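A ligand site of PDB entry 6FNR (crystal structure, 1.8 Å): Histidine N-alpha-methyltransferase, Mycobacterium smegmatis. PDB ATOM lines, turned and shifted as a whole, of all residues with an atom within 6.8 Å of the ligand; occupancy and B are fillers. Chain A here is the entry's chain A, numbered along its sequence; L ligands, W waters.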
ATOM      1  N   PHE A  40      25.743   5.789  -0.503  1.00  0.00           N
ATOM      2  CA  PHE A  40      25.149   6.361  -1.717  1.00  0.00           C
ATOM      3  C   PHE A  40      25.031   7.882  -1.638  1.00  0.00           C
ATOM      4  O   PHE A  40      25.048   8.548  -2.661  1.00  0.00           O
ATOM      5  CB  PHE A  40      23.733   5.817  -1.954  1.00  0.00           C
ATOM      6  CG  PHE A  40      23.676   4.444  -2.544  1.00  0.00           C
ATOM      7  CD1 PHE A  40      24.543   4.040  -3.546  1.00  0.00           C
ATOM      8  CD2 PHE A  40      22.707   3.555  -2.120  1.00  0.00           C
ATOM      9  CE1 PHE A  40      24.455   2.782  -4.098  1.00  0.00           C
ATOM     10  CE2 PHE A  40      22.615   2.298  -2.662  1.00  0.00           C
ATOM     11  CZ  PHE A  40      23.485   1.906  -3.653  1.00  0.00           C
ATOM     12  N   TYR A  41      24.907   8.419  -0.428  1.00  0.00           N
ATOM     13  CA  TYR A  41      24.338   9.756  -0.278  1.00  0.00           C
ATOM     14  C   TYR A  41      25.385  10.839  -0.041  1.00  0.00           C
ATOM     15  O   TYR A  41      25.276  11.647   0.888  1.00  0.00           O
ATOM     16  CB  TYR A  41      23.278   9.737   0.829  1.00  0.00           C
ATOM     17  CG  TYR A  41      22.131   8.817   0.477  1.00  0.00           C
ATOM     18  CD1 TYR A  41      21.093   9.236  -0.371  1.00  0.00           C
ATOM     19  CD2 TYR A  41      22.075   7.515   0.963  1.00  0.00           C
ATOM     20  CE1 TYR A  41      20.046   8.382  -0.702  1.00  0.00           C
ATOM     21  CE2 TYR A  41      21.029   6.652   0.634  1.00  0.00           C
ATOM     22  CZ  TYR A  41      20.024   7.097  -0.200  1.00  0.00           C
ATOM     23  OH  TYR A  41      18.986   6.245  -0.527  1.00  0.00           O
ATOM     24  N   PHE A  49      19.350  10.791  -6.131  1.00  0.00           N
ATOM     25  CA  PHE A  49      18.175  10.253  -5.477  1.00  0.00           C
ATOM     26  C   PHE A  49      16.987  11.213  -5.615  1.00  0.00           C
ATOM     27  O   PHE A  49      15.855  10.781  -5.809  1.00  0.00           O
ATOM     28  CB  PHE A  49      18.404   9.949  -3.995  1.00  0.00           C
ATOM     29  CG  PHE A  49      17.146   9.509  -3.304  1.00  0.00           C
ATOM     30  CD1 PHE A  49      16.613   8.271  -3.555  1.00  0.00           C
ATOM     31  CD2 PHE A  49      16.462  10.376  -2.473  1.00  0.00           C
ATOM     32  CE1 PHE A  49      15.426   7.875  -2.958  1.00  0.00           C
ATOM     33  CE2 PHE A  49      15.283   9.992  -1.873  1.00  0.00           C
ATOM     34  CZ  PHE A  49      14.761   8.735  -2.116  1.00  0.00           C
ATOM     35  N   ILE A  52      15.521  10.494  -8.839  1.00  0.00           N
ATOM     36  CA  ILE A  52      14.791   9.225  -8.770  1.00  0.00           C
ATOM     37  C   ILE A  52      13.358   9.424  -8.284  1.00  0.00           C
ATOM     38  O   ILE A  52      12.422   8.805  -8.820  1.00  0.00           O
ATOM     39  CB  ILE A  52      15.521   8.200  -7.855  1.00  0.00           C
ATOM     40  CG1 ILE A  52      16.787   7.682  -8.538  1.00  0.00           C
ATOM     41  CG2 ILE A  52      14.614   7.009  -7.501  1.00  0.00           C
ATOM     42  CD1 ILE A  52      17.688   6.816  -7.644  1.00  0.00           C
ATOM     43  N   TYR A  58       9.316   5.152 -10.499  1.00  0.00           N
ATOM     44  CA  TYR A  58       9.493   5.165  -9.043  1.00  0.00           C
ATOM     45  C   TYR A  58       8.275   5.781  -8.358  1.00  0.00           C
ATOM     46  O   TYR A  58       8.229   6.973  -8.037  1.00  0.00           O
ATOM     47  CB  TYR A  58      10.772   5.931  -8.664  1.00  0.00           C
ATOM     48  CG  TYR A  58      11.147   5.752  -7.210  1.00  0.00           C
ATOM     49  CD1 TYR A  58      11.712   4.566  -6.769  1.00  0.00           C
ATOM     50  CD2 TYR A  58      10.930   6.762  -6.280  1.00  0.00           C
ATOM     51  CE1 TYR A  58      12.056   4.383  -5.433  1.00  0.00           C
ATOM     52  CE2 TYR A  58      11.272   6.589  -4.946  1.00  0.00           C
ATOM     53  CZ  TYR A  58      11.827   5.407  -4.532  1.00  0.00           C
ATOM     54  OH  TYR A  58      12.158   5.252  -3.206  1.00  0.00           O
ATOM     55  N   PRO A  60       7.043   5.261  -5.263  1.00  0.00           N
ATOM     56  CA  PRO A  60       6.842   5.502  -3.823  1.00  0.00           C
ATOM     57  C   PRO A  60       6.671   6.969  -3.360  1.00  0.00           C
ATOM     58  O   PRO A  60       5.776   7.256  -2.551  1.00  0.00           O
ATOM     59  CB  PRO A  60       8.115   4.900  -3.195  1.00  0.00           C
ATOM     60  CG  PRO A  60       8.511   3.827  -4.140  1.00  0.00           C
ATOM     61  CD  PRO A  60       8.165   4.340  -5.513  1.00  0.00           C
ATOM     62  N   LEU A 162       9.549   8.611   6.922  1.00  0.00           N
ATOM     63  CA  LEU A 162       8.816   8.436   5.674  1.00  0.00           C
ATOM     64  C   LEU A 162       9.654   7.768   4.584  1.00  0.00           C
ATOM     65  O   LEU A 162      10.836   7.491   4.780  1.00  0.00           O
ATOM     66  CB  LEU A 162       8.311   9.793   5.177  1.00  0.00           C
ATOM     67  CG  LEU A 162       7.514  10.610   6.214  1.00  0.00           C
ATOM     68  CD1 LEU A 162       7.145  11.958   5.630  1.00  0.00           C
ATOM     69  CD2 LEU A 162       6.276   9.867   6.666  1.00  0.00           C
ATOM     70  N   GLY A 163       9.024   7.490   3.445  1.00  0.00           N
ATOM     71  CA  GLY A 163       9.747   7.068   2.258  1.00  0.00           C
ATOM     72  C   GLY A 163      10.060   5.568   2.165  1.00  0.00           C
ATOM     73  O   GLY A 163      10.639   5.124   1.189  1.00  0.00           O
ATOM     74  N   SER A 164       9.639   4.811   3.172  1.00  0.00           N
ATOM     75  CA  SER A 164       9.987   3.383   3.302  1.00  0.00           C
ATOM     76  C   SER A 164      11.501   3.189   3.456  1.00  0.00           C
ATOM     77  O   SER A 164      12.059   2.124   3.169  1.00  0.00           O
ATOM     78  CB  SER A 164       9.459   2.567   2.105  1.00  0.00           C
ATOM     79  OG  SER A 164       9.279   1.196   2.456  1.00  0.00           O
ATOM     80  N   THR A 165      12.165   4.216   3.989  1.00  0.00           N
ATOM     81  CA  THR A 165      13.576   4.111   4.317  1.00  0.00           C
ATOM     82  C   THR A 165      13.802   3.018   5.365  1.00  0.00           C
ATOM     83  O   THR A 165      14.868   2.408   5.425  1.00  0.00           O
ATOM     84  CB  THR A 165      14.120   5.465   4.821  1.00  0.00           C
ATOM     85  OG1 THR A 165      13.942   6.421   3.778  1.00  0.00           O
ATOM     86  CG2 THR A 165      15.601   5.384   5.182  1.00  0.00           C
ATOM     87  N   ILE A 166      12.788   2.738   6.163  1.00  0.00           N
ATOM     88  CA  ILE A 166      12.878   1.644   7.119  1.00  0.00           C
ATOM     89  C   ILE A 166      13.122   0.303   6.385  1.00  0.00           C
ATOM     90  O   ILE A 166      13.672  -0.624   6.982  1.00  0.00           O
ATOM     91  CB  ILE A 166      11.625   1.526   8.014  1.00  0.00           C
ATOM     92  CG1 ILE A 166      11.926   0.623   9.225  1.00  0.00           C
ATOM     93  CG2 ILE A 166      10.402   1.034   7.226  1.00  0.00           C
ATOM     94  CD1 ILE A 166      10.869   0.647  10.285  1.00  0.00           C
ATOM     95  N   GLY A 167      12.717   0.215   5.126  1.00  0.00           N
ATOM     96  CA  GLY A 167      12.944  -0.986   4.323  1.00  0.00           C
ATOM     97  C   GLY A 167      14.398  -1.283   3.972  1.00  0.00           C
ATOM     98  O   GLY A 167      14.718  -2.363   3.463  1.00  0.00           O
ATOM     99  N   ASN A 168      15.293  -0.328   4.225  1.00  0.00           N
ATOM    100  CA  ASN A 168      16.727  -0.551   4.024  1.00  0.00           C
ATOM    101  C   ASN A 168      17.350  -1.370   5.144  1.00  0.00           C
ATOM    102  O   ASN A 168      18.486  -1.861   5.012  1.00  0.00           O
ATOM    103  CB  ASN A 168      17.471   0.786   3.921  1.00  0.00           C
ATOM    104  CG  ASN A 168      17.257   1.485   2.595  1.00  0.00           C
ATOM    105  OD1 ASN A 168      16.850   0.880   1.594  1.00  0.00           O
ATOM    106  ND2 ASN A 168      17.538   2.781   2.575  1.00  0.00           N
ATOM    107  N   ASP A 196       6.506   0.851   2.044  1.00  0.00           N
ATOM    108  CA  ASP A 196       6.130   0.426   0.701  1.00  0.00           C
ATOM    109  C   ASP A 196       5.641  -1.020   0.766  1.00  0.00           C
ATOM    110  O   ASP A 196       6.186  -1.817   1.527  1.00  0.00           O
ATOM    111  CB  ASP A 196       7.315   0.577  -0.255  1.00  0.00           C
ATOM    112  CG  ASP A 196       6.919   0.467  -1.710  1.00  0.00           C
ATOM    113  OD1 ASP A 196       5.705   0.510  -1.999  1.00  0.00           O
ATOM    114  OD2 ASP A 196       7.817   0.356  -2.571  1.00  0.00           O
ATOM    115  N   ALA A 207      10.721  -0.061 -10.791  1.00  0.00           N
ATOM    116  CA  ALA A 207      10.931   1.102  -9.918  1.00  0.00           C
ATOM    117  C   ALA A 207      12.396   1.267  -9.535  1.00  0.00           C
ATOM    118  O   ALA A 207      12.811   2.372  -9.150  1.00  0.00           O
ATOM    119  CB  ALA A 207      10.062   0.998  -8.659  1.00  0.00           C
ATOM    120  N   TYR A 208      13.165   0.189  -9.622  1.00  0.00           N
ATOM    121  CA  TYR A 208      14.589   0.205  -9.256  1.00  0.00           C
ATOM    122  C   TYR A 208      15.507  -0.075 -10.459  1.00  0.00           C
ATOM    123  O   TYR A 208      16.686  -0.368 -10.297  1.00  0.00           O
ATOM    124  CB  TYR A 208      14.826  -0.820  -8.119  1.00  0.00           C
ATOM    125  CG  TYR A 208      14.119  -0.374  -6.860  1.00  0.00           C
ATOM    126  CD1 TYR A 208      12.762  -0.624  -6.669  1.00  0.00           C
ATOM    127  CD2 TYR A 208      14.796   0.342  -5.880  1.00  0.00           C
ATOM    128  CE1 TYR A 208      12.105  -0.191  -5.529  1.00  0.00           C
ATOM    129  CE2 TYR A 208      14.134   0.775  -4.731  1.00  0.00           C
ATOM    130  CZ  TYR A 208      12.798   0.502  -4.572  1.00  0.00           C
ATOM    131  OH  TYR A 208      12.123   0.930  -3.441  1.00  0.00           O
ATOM    132  N   THR A 215      18.646   5.268 -11.963  1.00  0.00           N
ATOM    133  CA  THR A 215      18.925   4.426 -10.802  1.00  0.00           C
ATOM    134  C   THR A 215      20.271   3.718 -10.972  1.00  0.00           C
ATOM    135  O   THR A 215      21.018   3.561 -10.008  1.00  0.00           O
ATOM    136  CB  THR A 215      17.822   3.398 -10.555  1.00  0.00           C
ATOM    137  OG1 THR A 215      16.575   4.070 -10.364  1.00  0.00           O
ATOM    138  CG2 THR A 215      18.136   2.606  -9.303  1.00  0.00           C
ATOM    139  N   PHE A 218      22.923   6.154  -9.947  1.00  0.00           N
ATOM    140  CA  PHE A 218      22.889   6.245  -8.484  1.00  0.00           C
ATOM    141  C   PHE A 218      23.633   5.087  -7.819  1.00  0.00           C
ATOM    142  O   PHE A 218      24.424   5.278  -6.881  1.00  0.00           O
ATOM    143  CB  PHE A 218      21.416   6.277  -8.056  1.00  0.00           C
ATOM    144  CG  PHE A 218      21.195   6.236  -6.574  1.00  0.00           C
ATOM    145  CD1 PHE A 218      21.446   7.349  -5.787  1.00  0.00           C
ATOM    146  CD2 PHE A 218      20.656   5.109  -5.982  1.00  0.00           C
ATOM    147  CE1 PHE A 218      21.213   7.327  -4.426  1.00  0.00           C
ATOM    148  CE2 PHE A 218      20.419   5.079  -4.610  1.00  0.00           C
ATOM    149  CZ  PHE A 218      20.689   6.181  -3.835  1.00  0.00           C
ATOM    150  N   ILE A 252      13.284  -5.933  -2.628  1.00  0.00           N
ATOM    151  CA  ILE A 252      14.072  -5.557  -3.789  1.00  0.00           C
ATOM    152  C   ILE A 252      15.527  -5.529  -3.374  1.00  0.00           C
ATOM    153  O   ILE A 252      15.847  -5.176  -2.233  1.00  0.00           O
ATOM    154  CB  ILE A 252      13.646  -4.178  -4.339  1.00  0.00           C
ATOM    155  CG1 ILE A 252      12.362  -4.308  -5.174  1.00  0.00           C
ATOM    156  CG2 ILE A 252      14.782  -3.508  -5.151  1.00  0.00           C
ATOM    157  CD1 ILE A 252      12.519  -5.024  -6.495  1.00  0.00           C
ATOM    158  N   MET A 254      19.454  -4.224  -4.970  1.00  0.00           N
ATOM    159  CA  MET A 254      20.316  -3.656  -6.013  1.00  0.00           C
ATOM    160  C   MET A 254      21.688  -4.299  -5.940  1.00  0.00           C
ATOM    161  O   MET A 254      22.273  -4.445  -4.857  1.00  0.00           O
ATOM    162  CB  MET A 254      20.437  -2.131  -5.892  1.00  0.00           C
ATOM    163  CG  MET A 254      19.111  -1.384  -5.987  1.00  0.00           C
ATOM    164  SD  MET A 254      19.271   0.289  -6.652  1.00  0.00           S
ATOM    165  CE  MET A 254      20.633   0.914  -5.717  1.00  0.00           C
ATOM    166  N   GLU A 284      22.270  -2.658  -1.960  1.00  0.00           N
ATOM    167  CA  GLU A 284      21.081  -2.178  -1.255  1.00  0.00           C
ATOM    168  C   GLU A 284      19.994  -3.244  -1.188  1.00  0.00           C
ATOM    169  O   GLU A 284      19.818  -4.007  -2.132  1.00  0.00           O
ATOM    170  CB  GLU A 284      20.520  -0.930  -1.939  1.00  0.00           C
ATOM    171  CG  GLU A 284      19.431  -0.215  -1.118  1.00  0.00           C
ATOM    172  CD  GLU A 284      18.819   0.967  -1.854  1.00  0.00           C
ATOM    173  OE1 GLU A 284      18.490   0.838  -3.047  1.00  0.00           O
ATOM    174  OE2 GLU A 284      18.659   2.034  -1.228  1.00  0.00           O
ATOM    175  N   VAL A 285      19.276  -3.293  -0.072  1.00  0.00           N
ATOM    176  CA  VAL A 285      18.006  -4.026  -0.022  1.00  0.00           C
ATOM    177  C   VAL A 285      16.905  -3.015   0.263  1.00  0.00           C
ATOM    178  O   VAL A 285      17.121  -1.999   0.929  1.00  0.00           O
ATOM    179  CB  VAL A 285      18.002  -5.152   1.048  1.00  0.00           C
ATOM    180  CG1 VAL A 285      19.145  -6.131   0.803  1.00  0.00           C
ATOM    181  CG2 VAL A 285      18.079  -4.591   2.437  1.00  0.00           C
ATOM    182  N   SER A 286      15.729  -3.286  -0.275  1.00  0.00           N
ATOM    183  CA  SER A 286      14.560  -2.462  -0.028  1.00  0.00           C
ATOM    184  C   SER A 286      13.387  -3.387   0.274  1.00  0.00           C
ATOM    185  O   SER A 286      12.688  -3.837  -0.633  1.00  0.00           O
ATOM    186  CB  SER A 286      14.286  -1.554  -1.226  1.00  0.00           C
ATOM    187  OG  SER A 286      13.178  -0.716  -0.994  1.00  0.00           O
ATOM    188  N   CYS A 287      13.209  -3.702   1.549  1.00  0.00           N
ATOM    189  CA  CYS A 287      12.174  -4.641   1.968  1.00  0.00           C
ATOM    190  C   CYS A 287      10.789  -4.055   1.691  1.00  0.00           C
ATOM    191  O   CYS A 287      10.578  -2.851   1.835  1.00  0.00           O
ATOM    192  CB  CYS A 287      12.339  -4.983   3.456  1.00  0.00           C
ATOM    193  SG  CYS A 287      13.939  -5.780   3.843  1.00  0.00           S
ATOM    194  N   LYS A 288       9.872  -4.917   1.281  1.00  0.00           N
ATOM    195  CA  LYS A 288       8.495  -4.515   0.995  1.00  0.00           C
ATOM    196  C   LYS A 288       7.587  -5.230   1.985  1.00  0.00           C
ATOM    197  O   LYS A 288       7.884  -6.361   2.396  1.00  0.00           O
ATOM    198  CB  LYS A 288       8.122  -4.824  -0.449  1.00  0.00           C
ATOM    199  CG  LYS A 288       9.053  -4.152  -1.468  1.00  0.00           C
ATOM    200  CD  LYS A 288       9.060  -2.619  -1.349  1.00  0.00           C
ATOM    201  CE  LYS A 288      10.153  -2.014  -2.210  1.00  0.00           C
ATOM    202  NZ  LYS A 288      10.345  -0.549  -1.956  1.00  0.00           N
HETATM  203  O1  LIG L   1      13.150   2.937  -2.434  1.00  0.00           O
HETATM  204  C1  LIG L   1      14.131   2.961  -1.651  1.00  0.00           C
HETATM  205  O2  LIG L   1      14.501   1.917  -1.077  1.00  0.00           O
HETATM  206  C2  LIG L   1      14.846   4.265  -1.382  1.00  0.00           C
HETATM  207 CL1  LIG L   1      14.925   4.486   0.350  1.00  0.00          CL
HETATM  208  C3  LIG L   1      16.257   4.248  -1.922  1.00  0.00           C
HETATM  209  C4  LIG L   1      16.324   3.875  -3.382  1.00  0.00           C
HETATM  210  C5  LIG L   1      15.564   4.409  -4.405  1.00  0.00           C
HETATM  211  N1  LIG L   1      15.960   3.787  -5.580  1.00  0.00           N
HETATM  212  C6  LIG L   1      16.953   2.893  -5.278  1.00  0.00           C
HETATM  213  N2  LIG L   1      17.179   2.946  -3.915  1.00  0.00           N
HETATM  214  O   HOH W   1      13.338   0.674   1.432  1.00  0.00           O
HETATM  215  O   HOH W   2      15.028   3.672  -8.201  1.00  0.00           O
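OH of Tyr 208 lies within hydrogen-bond range of O1 of the ligand (2.5 Å). OE1 of Glu 284 sits at hydrogen-bond distance from N2 of the ligand, at 2.6 Å. An oxygen (O1) of the ligand lies within hydrogen-bond range of the side-chain hydroxyl of Tyr 58 (2.6 Å). The side-chain hydroxyl (OG) of Ser 286 sits at hydrogen-bond distance from an oxygen (O2) of the ligand.
OG of Ser 286 sits at hydrogen-bond distance from OH of Tyr 208 (3.1 Å). The side-chain hydroxyl (OH) of Tyr 208 is in hydrogen-bond range of the side-chain amino group (NZ) of Lys 288 (2.7 Å). The backbone carbonyl oxygen (O) of Glu 284 is in hydrogen-bond range of the backbone NH (N) of Met 254 (2.9 Å). The side-chain amino group of Lys 288 is in hydrogen-bond range of the side-chain hydroxyl of Ser 286, at 3.0 Å. The backbone carbonyl oxygen of Ile 252 sits at hydrogen-bond distance from the backbone NH of Ser 286. The side-chain amide oxygen (OD1) of Asn 168 lies close to the backbone carbonyl oxygen (O) of Val 285, at 3.0 Å.
OH of Tyr 41 touches C3 of the ligand, at 3.7 Å. Phe 49 touches the ligand (CE1 to C5, 3.8 Å). CG2 of Ile 52 touches N1 of the ligand, 3.99 Å away. OD1 of Asn 168 touches O2 of the ligand (3.7 Å). Phe 218 touches the ligand (CE2 to N2, 3.9 Å). Met 254 touches the ligand (SD to C6, 3.7 Å). Of the 25 residues printed, 10 come within 4 Å of the ligand.
Water W2 lies within hydrogen-bond range of OG1 of Thr 215 (2.7 Å), O of Ala 207 (2.7 Å) and N1 of the ligand (2.8 Å). Water W1 lies within hydrogen-bond range of the backbone carbonyl oxygen of Ser 164 (2.6 Å), the side-chain hydroxyl of Ser 286 (2.8 Å) and an oxygen (O2) of the ligand (3.0 Å).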
